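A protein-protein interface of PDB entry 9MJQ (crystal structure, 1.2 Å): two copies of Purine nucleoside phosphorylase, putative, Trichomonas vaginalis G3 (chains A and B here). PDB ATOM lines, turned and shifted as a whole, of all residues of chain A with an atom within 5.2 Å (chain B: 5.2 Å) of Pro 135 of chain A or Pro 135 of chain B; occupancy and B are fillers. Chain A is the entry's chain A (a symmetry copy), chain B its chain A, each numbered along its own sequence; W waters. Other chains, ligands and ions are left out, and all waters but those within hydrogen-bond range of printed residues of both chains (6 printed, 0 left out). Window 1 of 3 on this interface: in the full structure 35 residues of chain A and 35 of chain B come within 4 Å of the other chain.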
ATOM      1  N   ALA A 117     -18.358   9.630  27.691  1.00  0.00           N
ATOM      2  CA  ALA A 117     -17.523   8.445  27.868  1.00  0.00           C
ATOM      3  C   ALA A 117     -16.650   8.719  29.082  1.00  0.00           C
ATOM      4  O   ALA A 117     -16.455   9.872  29.459  1.00  0.00           O
ATOM      5  CB  ALA A 117     -16.639   8.176  26.642  1.00  0.00           C
ATOM      6  N   SER A 118     -16.075   7.667  29.663  1.00  0.00           N
ATOM      7  CA  SER A 118     -15.265   7.829  30.866  1.00  0.00           C
ATOM      8  C   SER A 118     -14.002   6.992  30.760  1.00  0.00           C
ATOM      9  O   SER A 118     -14.071   5.786  30.516  1.00  0.00           O
ATOM     10  CB  SER A 118     -16.039   7.456  32.137  1.00  0.00           C
ATOM     11  OG  SER A 118     -15.370   7.955  33.290  1.00  0.00           O
ATOM     12  N   GLY A 119     -12.855   7.640  30.975  1.00  0.00           N
ATOM     13  CA  GLY A 119     -11.592   6.942  31.081  1.00  0.00           C
ATOM     14  C   GLY A 119     -11.463   6.299  32.447  1.00  0.00           C
ATOM     15  O   GLY A 119     -12.319   6.467  33.318  1.00  0.00           O
ATOM     16  N   ASP A 133      -8.000  -1.389  24.414  1.00  0.00           N
ATOM     17  CA  ASP A 133      -8.722  -0.213  24.877  1.00  0.00           C
ATOM     18  C   ASP A 133     -10.188  -0.341  24.494  1.00  0.00           C
ATOM     19  O   ASP A 133     -10.544  -0.302  23.303  1.00  0.00           O
ATOM     20  CB  ASP A 133      -8.186   1.089  24.287  1.00  0.00           C
ATOM     21  CG  ASP A 133      -6.871   1.539  24.878  1.00  0.00           C
ATOM     22  OD1 ASP A 133      -6.260   0.779  25.649  1.00  0.00           O
ATOM     23  OD2 ASP A 133      -6.455   2.684  24.587  1.00  0.00           O
ATOM     24  N   PHE A 134     -11.022  -0.430  25.513  1.00  0.00           N
ATOM     25  CA  PHE A 134     -12.472  -0.530  25.399  1.00  0.00           C
ATOM     26  C   PHE A 134     -13.031   0.761  25.985  1.00  0.00           C
ATOM     27  O   PHE A 134     -12.990   0.937  27.209  1.00  0.00           O
ATOM     28  CB  PHE A 134     -12.902  -1.742  26.231  1.00  0.00           C
ATOM     29  CG  PHE A 134     -14.397  -2.042  26.272  1.00  0.00           C
ATOM     30  CD1 PHE A 134     -15.374  -1.132  25.913  1.00  0.00           C
ATOM     31  CD2 PHE A 134     -14.803  -3.274  26.749  1.00  0.00           C
ATOM     32  CE1 PHE A 134     -16.732  -1.464  26.017  1.00  0.00           C
ATOM     33  CE2 PHE A 134     -16.137  -3.600  26.873  1.00  0.00           C
ATOM     34  CZ  PHE A 134     -17.107  -2.698  26.493  1.00  0.00           C
ATOM     35  N   PRO A 135     -13.554   1.686  25.179  1.00  0.00           N
ATOM     36  CA  PRO A 135     -14.046   2.948  25.740  1.00  0.00           C
ATOM     37  C   PRO A 135     -15.358   2.718  26.467  1.00  0.00           C
ATOM     38  O   PRO A 135     -16.296   2.155  25.898  1.00  0.00           O
ATOM     39  CB  PRO A 135     -14.246   3.825  24.500  1.00  0.00           C
ATOM     40  CG  PRO A 135     -14.576   2.859  23.417  1.00  0.00           C
ATOM     41  CD  PRO A 135     -13.747   1.622  23.724  1.00  0.00           C
ATOM     42  N   ALA A 136     -15.406   3.126  27.730  1.00  0.00           N
ATOM     43  CA  ALA A 136     -16.642   3.106  28.484  1.00  0.00           C
ATOM     44  C   ALA A 136     -17.485   4.268  27.974  1.00  0.00           C
ATOM     45  O   ALA A 136     -17.175   5.434  28.237  1.00  0.00           O
ATOM     46  CB  ALA A 136     -16.341   3.237  29.975  1.00  0.00           C
ATOM     47  N   THR A 137     -18.528   3.965  27.212  1.00  0.00           N
ATOM     48  CA  THR A 137     -19.221   4.951  26.399  1.00  0.00           C
ATOM     49  C   THR A 137     -20.689   4.987  26.803  1.00  0.00           C
ATOM     50  O   THR A 137     -21.357   3.944  26.844  1.00  0.00           O
ATOM     51  CB  THR A 137     -19.079   4.588  24.910  1.00  0.00           C
ATOM     52  OG1 THR A 137     -17.705   4.360  24.588  1.00  0.00           O
ATOM     53  CG2 THR A 137     -19.598   5.707  24.045  1.00  0.00           C
ATOM     54  N   LYS A 161     -16.024  14.126  28.412  1.00  0.00           N
ATOM     55  CA  LYS A 161     -15.451  12.935  29.017  1.00  0.00           C
ATOM     56  C   LYS A 161     -15.302  13.075  30.525  1.00  0.00           C
ATOM     57  O   LYS A 161     -14.872  14.117  31.032  1.00  0.00           O
ATOM     58  CB  LYS A 161     -14.043  12.671  28.467  1.00  0.00           C
ATOM     59  CG  LYS A 161     -13.972  12.373  26.972  1.00  0.00           C
ATOM     60  CD  LYS A 161     -12.531  12.098  26.513  1.00  0.00           C
ATOM     61  CE  LYS A 161     -11.579  13.254  26.803  1.00  0.00           C
ATOM     62  NZ  LYS A 161     -11.907  14.507  26.075  1.00  0.00           N
ATOM     63  N   ALA A 162     -15.557  11.980  31.226  1.00  0.00           N
ATOM     64  CA  ALA A 162     -15.183  11.827  32.624  1.00  0.00           C
ATOM     65  C   ALA A 162     -13.958  10.928  32.739  1.00  0.00           C
ATOM     66  O   ALA A 162     -13.531  10.294  31.781  1.00  0.00           O
ATOM     67  CB  ALA A 162     -16.341  11.229  33.423  1.00  0.00           C
ATOM     68  N   PHE A 184     -10.781  16.388  29.832  1.00  0.00           N
ATOM     69  CA  PHE A 184     -11.672  15.638  30.702  1.00  0.00           C
ATOM     70  C   PHE A 184     -12.342  16.615  31.653  1.00  0.00           C
ATOM     71  O   PHE A 184     -11.670  17.426  32.300  1.00  0.00           O
ATOM     72  CB  PHE A 184     -10.879  14.604  31.495  1.00  0.00           C
ATOM     73  CG  PHE A 184     -10.424  13.427  30.667  1.00  0.00           C
ATOM     74  CD1 PHE A 184      -9.298  13.493  29.862  1.00  0.00           C
ATOM     75  CD2 PHE A 184     -11.136  12.242  30.692  1.00  0.00           C
ATOM     76  CE1 PHE A 184      -8.901  12.396  29.127  1.00  0.00           C
ATOM     77  CE2 PHE A 184     -10.757  11.154  29.945  1.00  0.00           C
ATOM     78  CZ  PHE A 184      -9.635  11.224  29.159  1.00  0.00           C
ATOM     79  N   ASP A 199     -23.513  -2.371  28.078  1.00  0.00           N
ATOM     80  CA  ASP A 199     -23.253  -2.940  26.754  1.00  0.00           C
ATOM     81  C   ASP A 199     -23.431  -4.455  26.760  1.00  0.00           C
ATOM     82  O   ASP A 199     -24.044  -5.024  25.853  1.00  0.00           O
ATOM     83  CB  ASP A 199     -21.826  -2.640  26.300  1.00  0.00           C
ATOM     84  CG  ASP A 199     -21.582  -1.196  25.949  1.00  0.00           C
ATOM     85  OD1 ASP A 199     -22.544  -0.451  25.691  1.00  0.00           O
ATOM     86  OD2 ASP A 199     -20.387  -0.821  25.881  1.00  0.00           O
ATOM     87  N   ALA B 117     -17.686   6.651  20.110  1.00  0.00           N
ATOM     88  CA  ALA B 117     -16.347   6.465  20.666  1.00  0.00           C
ATOM     89  C   ALA B 117     -15.754   5.266  19.945  1.00  0.00           C
ATOM     90  O   ALA B 117     -16.486   4.451  19.387  1.00  0.00           O
ATOM     91  CB  ALA B 117     -16.384   6.199  22.177  1.00  0.00           C
ATOM     92  N   SER B 118     -14.431   5.120  20.002  1.00  0.00           N
ATOM     93  CA  SER B 118     -13.768   4.029  19.295  1.00  0.00           C
ATOM     94  C   SER B 118     -12.708   3.400  20.183  1.00  0.00           C
ATOM     95  O   SER B 118     -11.833   4.097  20.699  1.00  0.00           O
ATOM     96  CB  SER B 118     -13.141   4.494  17.975  1.00  0.00           C
ATOM     97  OG  SER B 118     -12.828   3.375  17.152  1.00  0.00           O
ATOM     98  N   GLY B 119     -12.783   2.076  20.329  1.00  0.00           N
ATOM     99  CA  GLY B 119     -11.745   1.321  20.998  1.00  0.00           C
ATOM    100  C   GLY B 119     -10.558   1.133  20.074  1.00  0.00           C
ATOM    101  O   GLY B 119     -10.587   1.524  18.906  1.00  0.00           O
ATOM    102  N   ASP B 133      -6.597   4.136  30.606  1.00  0.00           N
ATOM    103  CA  ASP B 133      -7.607   4.053  29.561  1.00  0.00           C
ATOM    104  C   ASP B 133      -8.144   5.445  29.269  1.00  0.00           C
ATOM    105  O   ASP B 133      -8.822   6.058  30.112  1.00  0.00           O
ATOM    106  CB  ASP B 133      -8.783   3.155  29.935  1.00  0.00           C
ATOM    107  CG  ASP B 133      -8.470   1.678  29.892  1.00  0.00           C
ATOM    108  OD1 ASP B 133      -7.296   1.310  29.722  1.00  0.00           O
ATOM    109  OD2 ASP B 133      -9.422   0.871  30.003  1.00  0.00           O
ATOM    110  N   PHE B 134      -7.885   5.897  28.057  1.00  0.00           N
ATOM    111  CA  PHE B 134      -8.321   7.187  27.536  1.00  0.00           C
ATOM    112  C   PHE B 134      -9.319   6.878  26.426  1.00  0.00           C
ATOM    113  O   PHE B 134      -8.907   6.417  25.354  1.00  0.00           O
ATOM    114  CB  PHE B 134      -7.077   7.886  26.977  1.00  0.00           C
ATOM    115  CG  PHE B 134      -7.292   9.265  26.362  1.00  0.00           C
ATOM    116  CD1 PHE B 134      -8.528   9.750  25.976  1.00  0.00           C
ATOM    117  CD2 PHE B 134      -6.182  10.053  26.122  1.00  0.00           C
ATOM    118  CE1 PHE B 134      -8.642  11.012  25.376  1.00  0.00           C
ATOM    119  CE2 PHE B 134      -6.285  11.286  25.513  1.00  0.00           C
ATOM    120  CZ  PHE B 134      -7.521  11.776  25.151  1.00  0.00           C
ATOM    121  N   PRO B 135     -10.619   7.104  26.618  1.00  0.00           N
ATOM    122  CA  PRO B 135     -11.582   6.760  25.567  1.00  0.00           C
ATOM    123  C   PRO B 135     -11.490   7.761  24.430  1.00  0.00           C
ATOM    124  O   PRO B 135     -11.576   8.970  24.654  1.00  0.00           O
ATOM    125  CB  PRO B 135     -12.931   6.861  26.286  1.00  0.00           C
ATOM    126  CG  PRO B 135     -12.714   7.898  27.331  1.00  0.00           C
ATOM    127  CD  PRO B 135     -11.276   7.704  27.787  1.00  0.00           C
ATOM    128  N   ALA B 136     -11.284   7.252  23.220  1.00  0.00           N
ATOM    129  CA  ALA B 136     -11.331   8.083  22.034  1.00  0.00           C
ATOM    130  C   ALA B 136     -12.800   8.379  21.766  1.00  0.00           C
ATOM    131  O   ALA B 136     -13.557   7.495  21.352  1.00  0.00           O
ATOM    132  CB  ALA B 136     -10.679   7.350  20.864  1.00  0.00           C
ATOM    133  N   THR B 137     -13.224   9.608  22.034  1.00  0.00           N
ATOM    134  CA  THR B 137     -14.633   9.949  22.139  1.00  0.00           C
ATOM    135  C   THR B 137     -14.957  11.044  21.132  1.00  0.00           C
ATOM    136  O   THR B 137     -14.284  12.083  21.092  1.00  0.00           O
ATOM    137  CB  THR B 137     -14.947  10.420  23.571  1.00  0.00           C
ATOM    138  OG1 THR B 137     -14.457   9.472  24.520  1.00  0.00           O
ATOM    139  CG2 THR B 137     -16.434  10.568  23.760  1.00  0.00           C
ATOM    140  N   LYS B 161     -20.365   2.373  19.273  1.00  0.00           N
ATOM    141  CA  LYS B 161     -18.916   2.288  19.349  1.00  0.00           C
ATOM    142  C   LYS B 161     -18.313   1.674  18.094  1.00  0.00           C
ATOM    143  O   LYS B 161     -18.819   0.680  17.561  1.00  0.00           O
ATOM    144  CB  LYS B 161     -18.485   1.392  20.517  1.00  0.00           C
ATOM    145  CG  LYS B 161     -18.880   1.894  21.904  1.00  0.00           C
ATOM    146  CD  LYS B 161     -18.388   0.950  23.013  1.00  0.00           C
ATOM    147  CE  LYS B 161     -18.917  -0.473  22.866  1.00  0.00           C
ATOM    148  NZ  LYS B 161     -20.394  -0.588  22.987  1.00  0.00           N
ATOM    149  N   ALA B 162     -17.169   2.208  17.692  1.00  0.00           N
ATOM    150  CA  ALA B 162     -16.298   1.575  16.714  1.00  0.00           C
ATOM    151  C   ALA B 162     -15.100   0.945  17.414  1.00  0.00           C
ATOM    152  O   ALA B 162     -14.859   1.157  18.596  1.00  0.00           O
ATOM    153  CB  ALA B 162     -15.816   2.600  15.687  1.00  0.00           C
ATOM    154  N   PHE B 184     -19.927  -3.473  19.765  1.00  0.00           N
ATOM    155  CA  PHE B 184     -19.201  -2.619  18.839  1.00  0.00           C
ATOM    156  C   PHE B 184     -19.810  -2.789  17.458  1.00  0.00           C
ATOM    157  O   PHE B 184     -19.981  -3.916  16.980  1.00  0.00           O
ATOM    158  CB  PHE B 184     -17.729  -3.015  18.810  1.00  0.00           C
ATOM    159  CG  PHE B 184     -16.967  -2.606  20.047  1.00  0.00           C
ATOM    160  CD1 PHE B 184     -17.017  -3.351  21.214  1.00  0.00           C
ATOM    161  CD2 PHE B 184     -16.197  -1.458  20.042  1.00  0.00           C
ATOM    162  CE1 PHE B 184     -16.300  -2.957  22.324  1.00  0.00           C
ATOM    163  CE2 PHE B 184     -15.499  -1.050  21.151  1.00  0.00           C
ATOM    164  CZ  PHE B 184     -15.545  -1.798  22.299  1.00  0.00           C
ATOM    165  N   ASP B 199      -9.158  16.524  20.859  1.00  0.00           N
ATOM    166  CA  ASP B 199      -9.188  16.949  22.260  1.00  0.00           C
ATOM    167  C   ASP B 199      -7.978  17.812  22.601  1.00  0.00           C
ATOM    168  O   ASP B 199      -8.105  18.848  23.259  1.00  0.00           O
ATOM    169  CB  ASP B 199      -9.181  15.743  23.197  1.00  0.00           C
ATOM    170  CG  ASP B 199     -10.463  14.954  23.199  1.00  0.00           C
ATOM    171  OD1 ASP B 199     -11.511  15.478  22.780  1.00  0.00           O
ATOM    172  OD2 ASP B 199     -10.421  13.799  23.683  1.00  0.00           O
HETATM  173  O   HOH W   1     -12.009   1.669  29.656  1.00  0.00           O
HETATM  174  O   HOH W   2      -8.112   4.564  23.505  1.00  0.00           O
HETATM  175  O   HOH W   3      -9.973  -1.024  28.059  1.00  0.00           O
HETATM  176  O   HOH W   4     -13.659  13.895  23.129  1.00  0.00           O
HETATM  177  O   HOH W   5     -21.761   1.993  24.882  1.00  0.00           O
HETATM  178  O   HOH W   6      -5.917   4.586  26.526  1.00  0.00           O
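Ala 117 of chain A touches Pro 135 of chain B (CB to CB, 3.95 Å).
Ala 117 of chain A touches Thr 137 of chain B.
Pro 135 of chain B touches Ser 118 of chain A.
Asp 133 of chain B touches Gly 119 of chain A (O to CA, 3.1 Å).
CD of Pro 135 of chain B touches CA of Gly 119 of chain A, 3.4 Å away.
Asp 133 of chain A touches Gly 119 of chain B.
Pro 135 of chain A touches Gly 119 of chain B.
Pro 135 of chain A touches Pro 135 of chain B.
Pro 135 of chain A touches Lys 161 of chain B.
Lys 161 of chain A touches Thr 137 of chain B (CD to OG1, 3.8 Å).
Water W4 lies within hydrogen-bond range of the side-chain carboxylate (OD1) of Asp 199 of chain B (2.7 Å), the backbone carbonyl oxygen (O) of Thr 137 of chain B (2.8 Å) and the side-chain amino group (NZ) of Lys 161 of chain A (3.5 Å).
Water W5 lies within hydrogen-bond range of OD1 of Asp 199 of chain A, O of Thr 137 of chain A and NZ of Lys 161 of chain B.
Water W2 bridges OD2 of Asp 133 of chain A (2.7 Å) and O of Phe 134 of chain B (2.7 Å).
Water W1 lies within hydrogen-bond range of the side-chain carboxylate of Asp 133 of chain B and the backbone carbonyl oxygen of Phe 134 of chain A.
Water W6 bridges the side-chain carboxylate of Asp 133 of chain A (2.8 Å) and the backbone NH of Phe 134 of chain B (2.8 Å).
Water W3 lies within hydrogen-bond range of OD2 of Asp 133 of chain B (2.8 Å) and N of Phe 134 of chain A (2.8 Å).
Of the 12 printed residues of chain A, 10 touch a printed residue of chain B.
Printed residues of chain A that touch a printed residue of chain B: Ala 117, Ser 118, Gly 119, Asp 133, Phe 134, Pro 135, Thr 137, Lys 161, Phe 184 and Asp 199.
Hydrophobic or aromatic side chains of chain B that line the printed part of chain A: Ala 117, Phe 134, Pro 135 and Phe 184.
Among the printed residues, 21 pairs touch across the chains.
Among the printed residues, Asp or Glu carboxylates within 4 Å of a Lys or Arg side-chain nitrogen of the other chain: Lys 161 of chain A with Asp 199 of chain B (2.9 Å) and Asp 199 of chain A with Lys 161 of chain B (2.9 Å).
The side-chain carboxylate (OD2) of Asp 199 of chain B lies within salt-bridge range of the side-chain amino group (NZ) of Lys 161 of chain A, at 2.9 Å.
The side-chain carboxylate of Asp 199 of chain A is in salt-bridge range of the side-chain amino group of Lys 161 of chain B (2.9 Å).
The side-chain hydroxyl (OG) of Ser 118 of chain A lies close to the backbone carbonyl oxygen (O) of Ala 162 of chain A.
N of Gly 119 of chain A lies within hydrogen-bond range of O of Ala 162 of chain A.
O of Ala 162 of chain B is in hydrogen-bond range of N of Gly 119 of chain B (2.9 Å).
The backbone NH of Ser 118 of chain B is in hydrogen-bond range of the backbone carbonyl oxygen of Ala 136 of chain B (2.9 Å).
The backbone carbonyl oxygen (O) of Pro 135 of chain B is in hydrogen-bond range of the side-chain hydroxyl (OG1) of Thr 137 of chain B.
OG of Ser 118 of chain B lies close to O of Ala 162 of chain B (3.3 Å).
Of the printed residues of chain B, Gly 119 of chain A touches Asp 133 and Pro 135.
Printed residues of chain B within 4 Å of Asp 133 of chain A: Gly 119 (3.1 Å).
Of the printed residues of chain B, Pro 135 of chain A touches Ala 117 (3.95 Å), Ser 118 (3.8 Å), Gly 119 (3.4 Å), Pro 135 (3.8 Å) and Lys 161 (3.8 Å).
Ala 162 of chain A touches none of the printed residues of chain B.
Printed residues of chain B within 4 Å of Asp 199 of chain A: Lys 161.
Of the printed residues of chain A, Lys 161 of chain B touches Phe 134 (3.96 Å), Pro 135 (3.8 Å), Thr 137 (3.8 Å) and Asp 199 (2.9 Å).
Of the printed residues of chain A, Asp 199 of chain B touches Lys 161.
The nearest printed residue of chain A that does not touch Pro 135 of chain B is Phe 184 of chain A (4.1 Å).
The nearest printed residue of chain B that does not touch Asp 133 of chain A is Asp 133 of chain B (4.2 Å).
Ser 118 of chain A touches Pro 135 of chain B, and with the chains exchanged Pro 135 of chain A touches Ser 118 of chain B.
Gly 119 of chain A touches Asp 133 of chain B, and with the chains exchanged Asp 133 of chain A touches Gly 119 of chain B.
Pro 135 of chain A touches its own counterpart, Pro 135 of chain B.
Lys 161 of chain A touches Asp 199 of chain B, and with the chains exchanged Asp 199 of chain A touches Lys 161 of chain B.
Positions printed for both chains: 117, 118, 119, 133, 134, 135, 136, 137, 161, 162, 184 and 199.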
